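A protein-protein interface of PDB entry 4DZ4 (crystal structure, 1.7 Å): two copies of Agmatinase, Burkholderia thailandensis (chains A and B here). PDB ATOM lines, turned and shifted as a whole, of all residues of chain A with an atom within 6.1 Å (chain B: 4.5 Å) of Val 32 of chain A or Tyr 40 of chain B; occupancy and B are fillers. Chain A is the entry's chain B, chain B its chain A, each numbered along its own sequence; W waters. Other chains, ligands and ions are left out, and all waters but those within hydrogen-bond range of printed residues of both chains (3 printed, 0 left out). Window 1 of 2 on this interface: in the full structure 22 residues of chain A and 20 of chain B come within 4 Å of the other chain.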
ATOM      1  N   GLY A  11      15.765 -22.839  25.317  1.00  0.00           N
ATOM      2  CA  GLY A  11      14.590 -22.637  24.468  1.00  0.00           C
ATOM      3  C   GLY A  11      14.780 -23.078  23.029  1.00  0.00           C
ATOM      4  O   GLY A  11      15.868 -22.931  22.457  1.00  0.00           O
ATOM      5  N   ASP A  12      13.721 -23.625  22.446  1.00  0.00           N
ATOM      6  CA  ASP A  12      13.645 -23.922  21.003  1.00  0.00           C
ATOM      7  C   ASP A  12      14.683 -24.948  20.573  1.00  0.00           C
ATOM      8  O   ASP A  12      15.238 -24.866  19.489  1.00  0.00           O
ATOM      9  CB  ASP A  12      13.758 -22.627  20.176  1.00  0.00           C
ATOM     10  CG  ASP A  12      12.587 -21.712  20.402  1.00  0.00           C
ATOM     11  OD1 ASP A  12      11.460 -22.229  20.393  1.00  0.00           O
ATOM     12  OD2 ASP A  12      12.798 -20.491  20.554  1.00  0.00           O
ATOM     13  N   GLY A  13      14.919 -25.930  21.433  1.00  0.00           N
ATOM     14  CA  GLY A  13      15.852 -27.021  21.122  1.00  0.00           C
ATOM     15  C   GLY A  13      15.537 -27.775  19.831  1.00  0.00           C
ATOM     16  O   GLY A  13      16.459 -28.181  19.142  1.00  0.00           O
ATOM     17  N   ALA A  14      14.248 -27.924  19.491  1.00  0.00           N
ATOM     18  CA  ALA A  14      13.821 -28.644  18.293  1.00  0.00           C
ATOM     19  C   ALA A  14      14.424 -28.088  16.994  1.00  0.00           C
ATOM     20  O   ALA A  14      14.559 -28.810  15.992  1.00  0.00           O
ATOM     21  CB  ALA A  14      12.289 -28.642  18.220  1.00  0.00           C
ATOM     22  N   ILE A  15      14.794 -26.810  17.005  1.00  0.00           N
ATOM     23  CA  ILE A  15      15.318 -26.155  15.816  1.00  0.00           C
ATOM     24  C   ILE A  15      16.770 -25.689  15.988  1.00  0.00           C
ATOM     25  O   ILE A  15      17.373 -25.230  15.029  1.00  0.00           O
ATOM     26  CB  ILE A  15      14.401 -24.981  15.326  1.00  0.00           C
ATOM     27  CG1 ILE A  15      14.314 -23.828  16.360  1.00  0.00           C
ATOM     28  CG2 ILE A  15      13.022 -25.544  14.913  1.00  0.00           C
ATOM     29  CD1 ILE A  15      13.711 -22.512  15.838  1.00  0.00           C
ATOM     30  N   GLU A  26      13.673 -25.874  28.292  1.00  0.00           N
ATOM     31  CA  GLU A  26      12.550 -25.122  27.712  1.00  0.00           C
ATOM     32  C   GLU A  26      11.683 -24.507  28.809  1.00  0.00           C
ATOM     33  O   GLU A  26      11.552 -25.084  29.882  1.00  0.00           O
ATOM     34  CB  GLU A  26      11.638 -26.055  26.879  1.00  0.00           C
ATOM     35  CG  GLU A  26      12.376 -26.791  25.772  1.00  0.00           C
ATOM     36  CD  GLU A  26      12.427 -26.035  24.449  1.00  0.00           C
ATOM     37  OE1 GLU A  26      12.003 -24.853  24.365  1.00  0.00           O
ATOM     38  OE2 GLU A  26      12.918 -26.640  23.468  1.00  0.00           O
ATOM     39  N   ALA A  30       6.241 -22.472  26.237  1.00  0.00           N
ATOM     40  CA  ALA A  30       6.726 -21.813  25.021  1.00  0.00           C
ATOM     41  C   ALA A  30       7.614 -22.780  24.244  1.00  0.00           C
ATOM     42  O   ALA A  30       7.685 -23.977  24.568  1.00  0.00           O
ATOM     43  CB  ALA A  30       7.477 -20.528  25.380  1.00  0.00           C
ATOM     44  N   GLY A  31       8.304 -22.269  23.231  1.00  0.00           N
ATOM     45  CA  GLY A  31       9.268 -23.089  22.501  1.00  0.00           C
ATOM     46  C   GLY A  31       8.673 -23.907  21.368  1.00  0.00           C
ATOM     47  O   GLY A  31       7.483 -24.228  21.377  1.00  0.00           O
ATOM     48  N   VAL A  32       9.504 -24.284  20.390  1.00  0.00           N
ATOM     49  CA  VAL A  32       8.982 -25.022  19.209  1.00  0.00           C
ATOM     50  C   VAL A  32       8.352 -26.348  19.654  1.00  0.00           C
ATOM     51  O   VAL A  32       8.919 -27.082  20.458  1.00  0.00           O
ATOM     52  CB  VAL A  32      10.057 -25.250  18.145  1.00  0.00           C
ATOM     53  CG1 VAL A  32       9.511 -26.149  17.031  1.00  0.00           C
ATOM     54  CG2 VAL A  32      10.529 -23.921  17.565  1.00  0.00           C
ATOM     55  N   LEU A  33       7.134 -26.605  19.161  1.00  0.00           N
ATOM     56  CA  LEU A  33       6.319 -27.724  19.644  1.00  0.00           C
ATOM     57  C   LEU A  33       6.459 -28.992  18.771  1.00  0.00           C
ATOM     58  O   LEU A  33       5.466 -29.526  18.262  1.00  0.00           O
ATOM     59  CB  LEU A  33       4.833 -27.296  19.707  1.00  0.00           C
ATOM     60  CG  LEU A  33       4.501 -26.094  20.610  1.00  0.00           C
ATOM     61  CD1 LEU A  33       3.067 -25.599  20.377  1.00  0.00           C
ATOM     62  CD2 LEU A  33       4.750 -26.403  22.098  1.00  0.00           C
ATOM     63  N   SER A  34       7.682 -29.509  18.625  1.00  0.00           N
ATOM     64  CA  SER A  34       7.840 -30.856  18.043  1.00  0.00           C
ATOM     65  C   SER A  34       7.556 -31.893  19.132  1.00  0.00           C
ATOM     66  O   SER A  34       7.458 -31.548  20.315  1.00  0.00           O
ATOM     67  CB  SER A  34       9.268 -31.044  17.532  1.00  0.00           C
ATOM     68  OG  SER A  34      10.134 -30.940  18.652  1.00  0.00           O
ATOM     69  N   ARG A  37       9.902 -32.220  22.059  1.00  0.00           N
ATOM     70  CA  ARG A  37      10.967 -31.261  21.681  1.00  0.00           C
ATOM     71  C   ARG A  37      12.085 -31.829  20.824  1.00  0.00           C
ATOM     72  O   ARG A  37      13.138 -31.207  20.732  1.00  0.00           O
ATOM     73  CB  ARG A  37      11.614 -30.580  22.914  1.00  0.00           C
ATOM     74  CG  ARG A  37      10.619 -30.085  23.964  1.00  0.00           C
ATOM     75  CD  ARG A  37       9.712 -28.992  23.420  1.00  0.00           C
ATOM     76  NE  ARG A  37       9.064 -28.346  24.566  1.00  0.00           N
ATOM     77  CZ  ARG A  37       8.441 -27.174  24.522  1.00  0.00           C
ATOM     78  NH1 ARG A  37       8.320 -26.519  23.374  1.00  0.00           N
ATOM     79  NH2 ARG A  37       7.945 -26.654  25.642  1.00  0.00           N
ATOM     80  N   TYR A  40      13.395 -31.281  14.768  1.00  0.00           N
ATOM     81  CA  TYR A  40      12.681 -31.296  13.487  1.00  0.00           C
ATOM     82  C   TYR A  40      13.659 -31.471  12.338  1.00  0.00           C
ATOM     83  O   TYR A  40      14.493 -30.588  12.072  1.00  0.00           O
ATOM     84  CB  TYR A  40      11.961 -29.962  13.272  1.00  0.00           C
ATOM     85  CG  TYR A  40      10.526 -29.881  13.748  1.00  0.00           C
ATOM     86  CD1 TYR A  40       9.615 -30.940  13.554  1.00  0.00           C
ATOM     87  CD2 TYR A  40      10.054 -28.704  14.332  1.00  0.00           C
ATOM     88  CE1 TYR A  40       8.297 -30.826  13.985  1.00  0.00           C
ATOM     89  CE2 TYR A  40       8.715 -28.569  14.727  1.00  0.00           C
ATOM     90  CZ  TYR A  40       7.859 -29.622  14.547  1.00  0.00           C
ATOM     91  OH  TYR A  40       6.555 -29.479  14.941  1.00  0.00           O
ATOM     92  N   ALA B  14       8.428 -24.897   6.780  1.00  0.00           N
ATOM     93  CA  ALA B  14       9.137 -24.150   7.844  1.00  0.00           C
ATOM     94  C   ALA B  14      10.478 -24.782   8.251  1.00  0.00           C
ATOM     95  O   ALA B  14      11.364 -24.098   8.802  1.00  0.00           O
ATOM     96  CB  ALA B  14       8.269 -24.009   9.064  1.00  0.00           C
ATOM     97  N   ILE B  15      10.612 -26.082   8.020  1.00  0.00           N
ATOM     98  CA  ILE B  15      11.828 -26.766   8.433  1.00  0.00           C
ATOM     99  C   ILE B  15      12.566 -27.341   7.222  1.00  0.00           C
ATOM    100  O   ILE B  15      13.622 -27.963   7.363  1.00  0.00           O
ATOM    101  CB  ILE B  15      11.551 -27.877   9.488  1.00  0.00           C
ATOM    102  CG1 ILE B  15      10.619 -28.968   8.906  1.00  0.00           C
ATOM    103  CG2 ILE B  15      11.031 -27.253  10.792  1.00  0.00           C
ATOM    104  CD1 ILE B  15      10.515 -30.260   9.718  1.00  0.00           C
ATOM    105  N   VAL B  32       4.473 -28.119  10.206  1.00  0.00           N
ATOM    106  CA  VAL B  32       5.122 -27.383  11.283  1.00  0.00           C
ATOM    107  C   VAL B  32       4.475 -26.028  11.480  1.00  0.00           C
ATOM    108  O   VAL B  32       4.236 -25.310  10.507  1.00  0.00           O
ATOM    109  CB  VAL B  32       6.645 -27.249  11.027  1.00  0.00           C
ATOM    110  CG1 VAL B  32       7.263 -26.365  12.106  1.00  0.00           C
ATOM    111  CG2 VAL B  32       7.285 -28.627  11.083  1.00  0.00           C
ATOM    112  N   LEU B  33       4.202 -25.664  12.744  1.00  0.00           N
ATOM    113  CA  LEU B  33       3.375 -24.510  13.047  1.00  0.00           C
ATOM    114  C   LEU B  33       4.171 -23.267  13.414  1.00  0.00           C
ATOM    115  O   LEU B  33       3.951 -22.658  14.471  1.00  0.00           O
ATOM    116  CB  LEU B  33       2.389 -24.839  14.185  1.00  0.00           C
ATOM    117  CG  LEU B  33       1.387 -25.968  13.830  1.00  0.00           C
ATOM    118  CD1 LEU B  33       0.656 -26.386  15.109  1.00  0.00           C
ATOM    119  CD2 LEU B  33       0.381 -25.511  12.773  1.00  0.00           C
ATOM    120  N   SER B  34       5.084 -22.857  12.537  1.00  0.00           N
ATOM    121  CA  SER B  34       5.745 -21.548  12.730  1.00  0.00           C
ATOM    122  C   SER B  34       4.790 -20.459  12.227  1.00  0.00           C
ATOM    123  O   SER B  34       3.773 -20.744  11.565  1.00  0.00           O
ATOM    124  CB  SER B  34       7.031 -21.501  11.947  1.00  0.00           C
ATOM    125  OG  SER B  34       6.711 -21.593  10.559  1.00  0.00           O
ATOM    126  N   ARG B  38       6.674 -19.640   8.242  1.00  0.00           N
ATOM    127  CA  ARG B  38       7.986 -19.110   7.855  1.00  0.00           C
ATOM    128  C   ARG B  38       9.127 -19.956   8.408  1.00  0.00           C
ATOM    129  O   ARG B  38       8.961 -20.678   9.398  1.00  0.00           O
ATOM    130  CB  ARG B  38       8.131 -17.661   8.307  1.00  0.00           C
ATOM    131  CG  ARG B  38       7.108 -16.706   7.723  1.00  0.00           C
ATOM    132  CD  ARG B  38       7.332 -16.531   6.250  1.00  0.00           C
ATOM    133  NE  ARG B  38       6.756 -17.569   5.430  1.00  0.00           N
ATOM    134  CZ  ARG B  38       7.303 -18.025   4.281  1.00  0.00           C
ATOM    135  NH1 ARG B  38       8.457 -17.601   3.822  1.00  0.00           N
ATOM    136  NH2 ARG B  38       6.684 -18.948   3.582  1.00  0.00           N
ATOM    137  N   ASN B  39      10.305 -19.878   7.778  1.00  0.00           N
ATOM    138  CA  ASN B  39      11.420 -20.710   8.213  1.00  0.00           C
ATOM    139  C   ASN B  39      11.717 -20.507   9.710  1.00  0.00           C
ATOM    140  O   ASN B  39      11.861 -19.372  10.184  1.00  0.00           O
ATOM    141  CB  ASN B  39      12.704 -20.352   7.456  1.00  0.00           C
ATOM    142  CG  ASN B  39      12.668 -20.730   6.000  1.00  0.00           C
ATOM    143  OD1 ASN B  39      11.627 -21.043   5.441  1.00  0.00           O
ATOM    144  ND2 ASN B  39      13.840 -20.717   5.371  1.00  0.00           N
ATOM    145  N   TYR B  40      11.812 -21.607  10.444  1.00  0.00           N
ATOM    146  CA  TYR B  40      12.293 -21.564  11.817  1.00  0.00           C
ATOM    147  C   TYR B  40      13.816 -21.471  11.779  1.00  0.00           C
ATOM    148  O   TYR B  40      14.482 -22.405  11.344  1.00  0.00           O
ATOM    149  CB  TYR B  40      11.925 -22.863  12.532  1.00  0.00           C
ATOM    150  CG  TYR B  40      10.650 -22.829  13.365  1.00  0.00           C
ATOM    151  CD1 TYR B  40      10.337 -21.752  14.203  1.00  0.00           C
ATOM    152  CD2 TYR B  40       9.790 -23.937  13.362  1.00  0.00           C
ATOM    153  CE1 TYR B  40       9.164 -21.738  14.979  1.00  0.00           C
ATOM    154  CE2 TYR B  40       8.633 -23.956  14.138  1.00  0.00           C
ATOM    155  CZ  TYR B  40       8.337 -22.875  14.962  1.00  0.00           C
ATOM    156  OH  TYR B  40       7.199 -22.909  15.727  1.00  0.00           O
ATOM    157  N   THR B  41      14.354 -20.343  12.224  1.00  0.00           N
ATOM    158  CA  THR B  41      15.816 -20.147  12.180  1.00  0.00           C
ATOM    159  C   THR B  41      16.232 -18.995  13.074  1.00  0.00           C
ATOM    160  O   THR B  41      15.424 -18.109  13.371  1.00  0.00           O
ATOM    161  CB  THR B  41      16.335 -19.905  10.745  1.00  0.00           C
ATOM    162  OG1 THR B  41      17.763 -19.772  10.777  1.00  0.00           O
ATOM    163  CG2 THR B  41      15.732 -18.632  10.121  1.00  0.00           C
ATOM    164  N   ARG B  74       0.543 -18.469  16.381  1.00  0.00           N
ATOM    165  CA  ARG B  74       1.167 -19.314  15.373  1.00  0.00           C
ATOM    166  C   ARG B  74       0.171 -20.337  14.812  1.00  0.00           C
ATOM    167  O   ARG B  74       0.015 -20.439  13.597  1.00  0.00           O
ATOM    168  CB  ARG B  74       2.379 -20.043  15.960  1.00  0.00           C
ATOM    169  CG  ARG B  74       3.564 -19.084  16.177  1.00  0.00           C
ATOM    170  CD  ARG B  74       4.768 -19.851  16.696  1.00  0.00           C
ATOM    171  NE  ARG B  74       5.973 -19.022  16.769  1.00  0.00           N
ATOM    172  CZ  ARG B  74       6.504 -18.552  17.894  1.00  0.00           C
ATOM    173  NH1 ARG B  74       5.947 -18.823  19.074  1.00  0.00           N
ATOM    174  NH2 ARG B  74       7.626 -17.801  17.838  1.00  0.00           N
ATOM    175  N   ASP B 100      10.686 -17.056  11.509  1.00  0.00           N
ATOM    176  CA  ASP B 100      10.218 -17.276  12.865  1.00  0.00           C
ATOM    177  C   ASP B 100      11.423 -17.701  13.726  1.00  0.00           C
ATOM    178  O   ASP B 100      11.986 -18.783  13.533  1.00  0.00           O
ATOM    179  CB  ASP B 100       9.116 -18.344  12.906  1.00  0.00           C
ATOM    180  CG  ASP B 100       8.370 -18.360  14.241  1.00  0.00           C
ATOM    181  OD1 ASP B 100       8.984 -17.994  15.272  1.00  0.00           O
ATOM    182  OD2 ASP B 100       7.154 -18.680  14.264  1.00  0.00           O
HETATM  183  O   HOH W   1      15.509 -29.296   9.857  1.00  0.00           O
HETATM  184  O   HOH W   2       5.913 -25.146  16.888  1.00  0.00           O
HETATM  185  O   HOH W   3       5.004 -27.196  15.138  1.00  0.00           O
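The backbone carbonyl oxygen (O) of Ala 14 of chain B lies within hydrogen-bond range of the backbone NH (N) of Tyr 40 of chain B.
OH of Tyr 40 of chain B is in hydrogen-bond range of O of Leu 33 of chain B, at 3.5 Å.
OD1 of Asp 12 of chain A sits at hydrogen-bond distance from N of Val 32 of chain A, 2.8 Å away.
O of Ala 14 of chain A is in hydrogen-bond range of N of Tyr 40 of chain A, 3.0 Å away.
The guanidinium group (NH1) of Arg 37 of chain A is in hydrogen-bond range of the backbone carbonyl oxygen (O) of Val 32 of chain A, 3.0 Å away.
The backbone carbonyl oxygen (O) of Leu 33 of chain A lies within hydrogen-bond range of the side-chain hydroxyl (OH) of Tyr 40 of chain A (3.5 Å).
Among the printed residues, pairs that only touch across the chains: Ile 15 of chain A with Tyr 40 of chain B (3.7 Å), Val 32 of chain A with Tyr 40 of chain B (3.6 Å), Tyr 40 of chain A with Ile 15 of chain B (3.8 Å) and Tyr 40 of chain A with Val 32 of chain B (3.6 Å).
Ile 15 of chain A touches Tyr 40 of chain B, and with the chains exchanged Tyr 40 of chain A touches Ile 15 of chain B.
Val 32 of chain A touches Tyr 40 of chain B, and with the chains exchanged Tyr 40 of chain A touches Val 32 of chain B.
Positions printed for both chains: 14, 15, 32, 33, 34 and 40.
Of the 4 pairs that touch across the chains among the printed residues, 4 have their exchanged pair printed and touching as well.
Water W1 bridges the backbone carbonyl oxygen of Tyr 40 of chain A (2.8 Å) and the backbone carbonyl oxygen of Ile 15 of chain B (3.4 Å).
Water W3 lies within hydrogen-bond range of OH of Tyr 40 of chain A (2.8 Å) and N of Leu 33 of chain B (3.0 Å).
Water W2 bridges OH of Tyr 40 of chain B (2.8 Å) and N of Leu 33 of chain A (3.0 Å).
Val 32 of chain A touches one residue of chain B.
Tyr 40 of chain B touches just these residues of chain A: Ile 15 (3.7 Å) and Val 32 (3.6 Å).
Of the printed residues of chain A, Ile 15 of chain B touches Tyr 40 (3.8 Å).
Printed residues of chain A within 4 Å of Val 32 of chain B: Tyr 40.
Of the printed residues of chain B, Ile 15 of chain A touches Tyr 40 (3.7 Å).
Ala 14 of chain B touches none of the printed residues of chain A.
Printed residues of chain A that touch a printed residue of chain B: Ile 15, Val 32 and Tyr 40.
Among the printed residues, 4 pairs touch across the chains.
Among the printed residues, no Asp or Glu carboxylate lies within 4 Å of a Lys or Arg side-chain nitrogen of the other chain.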
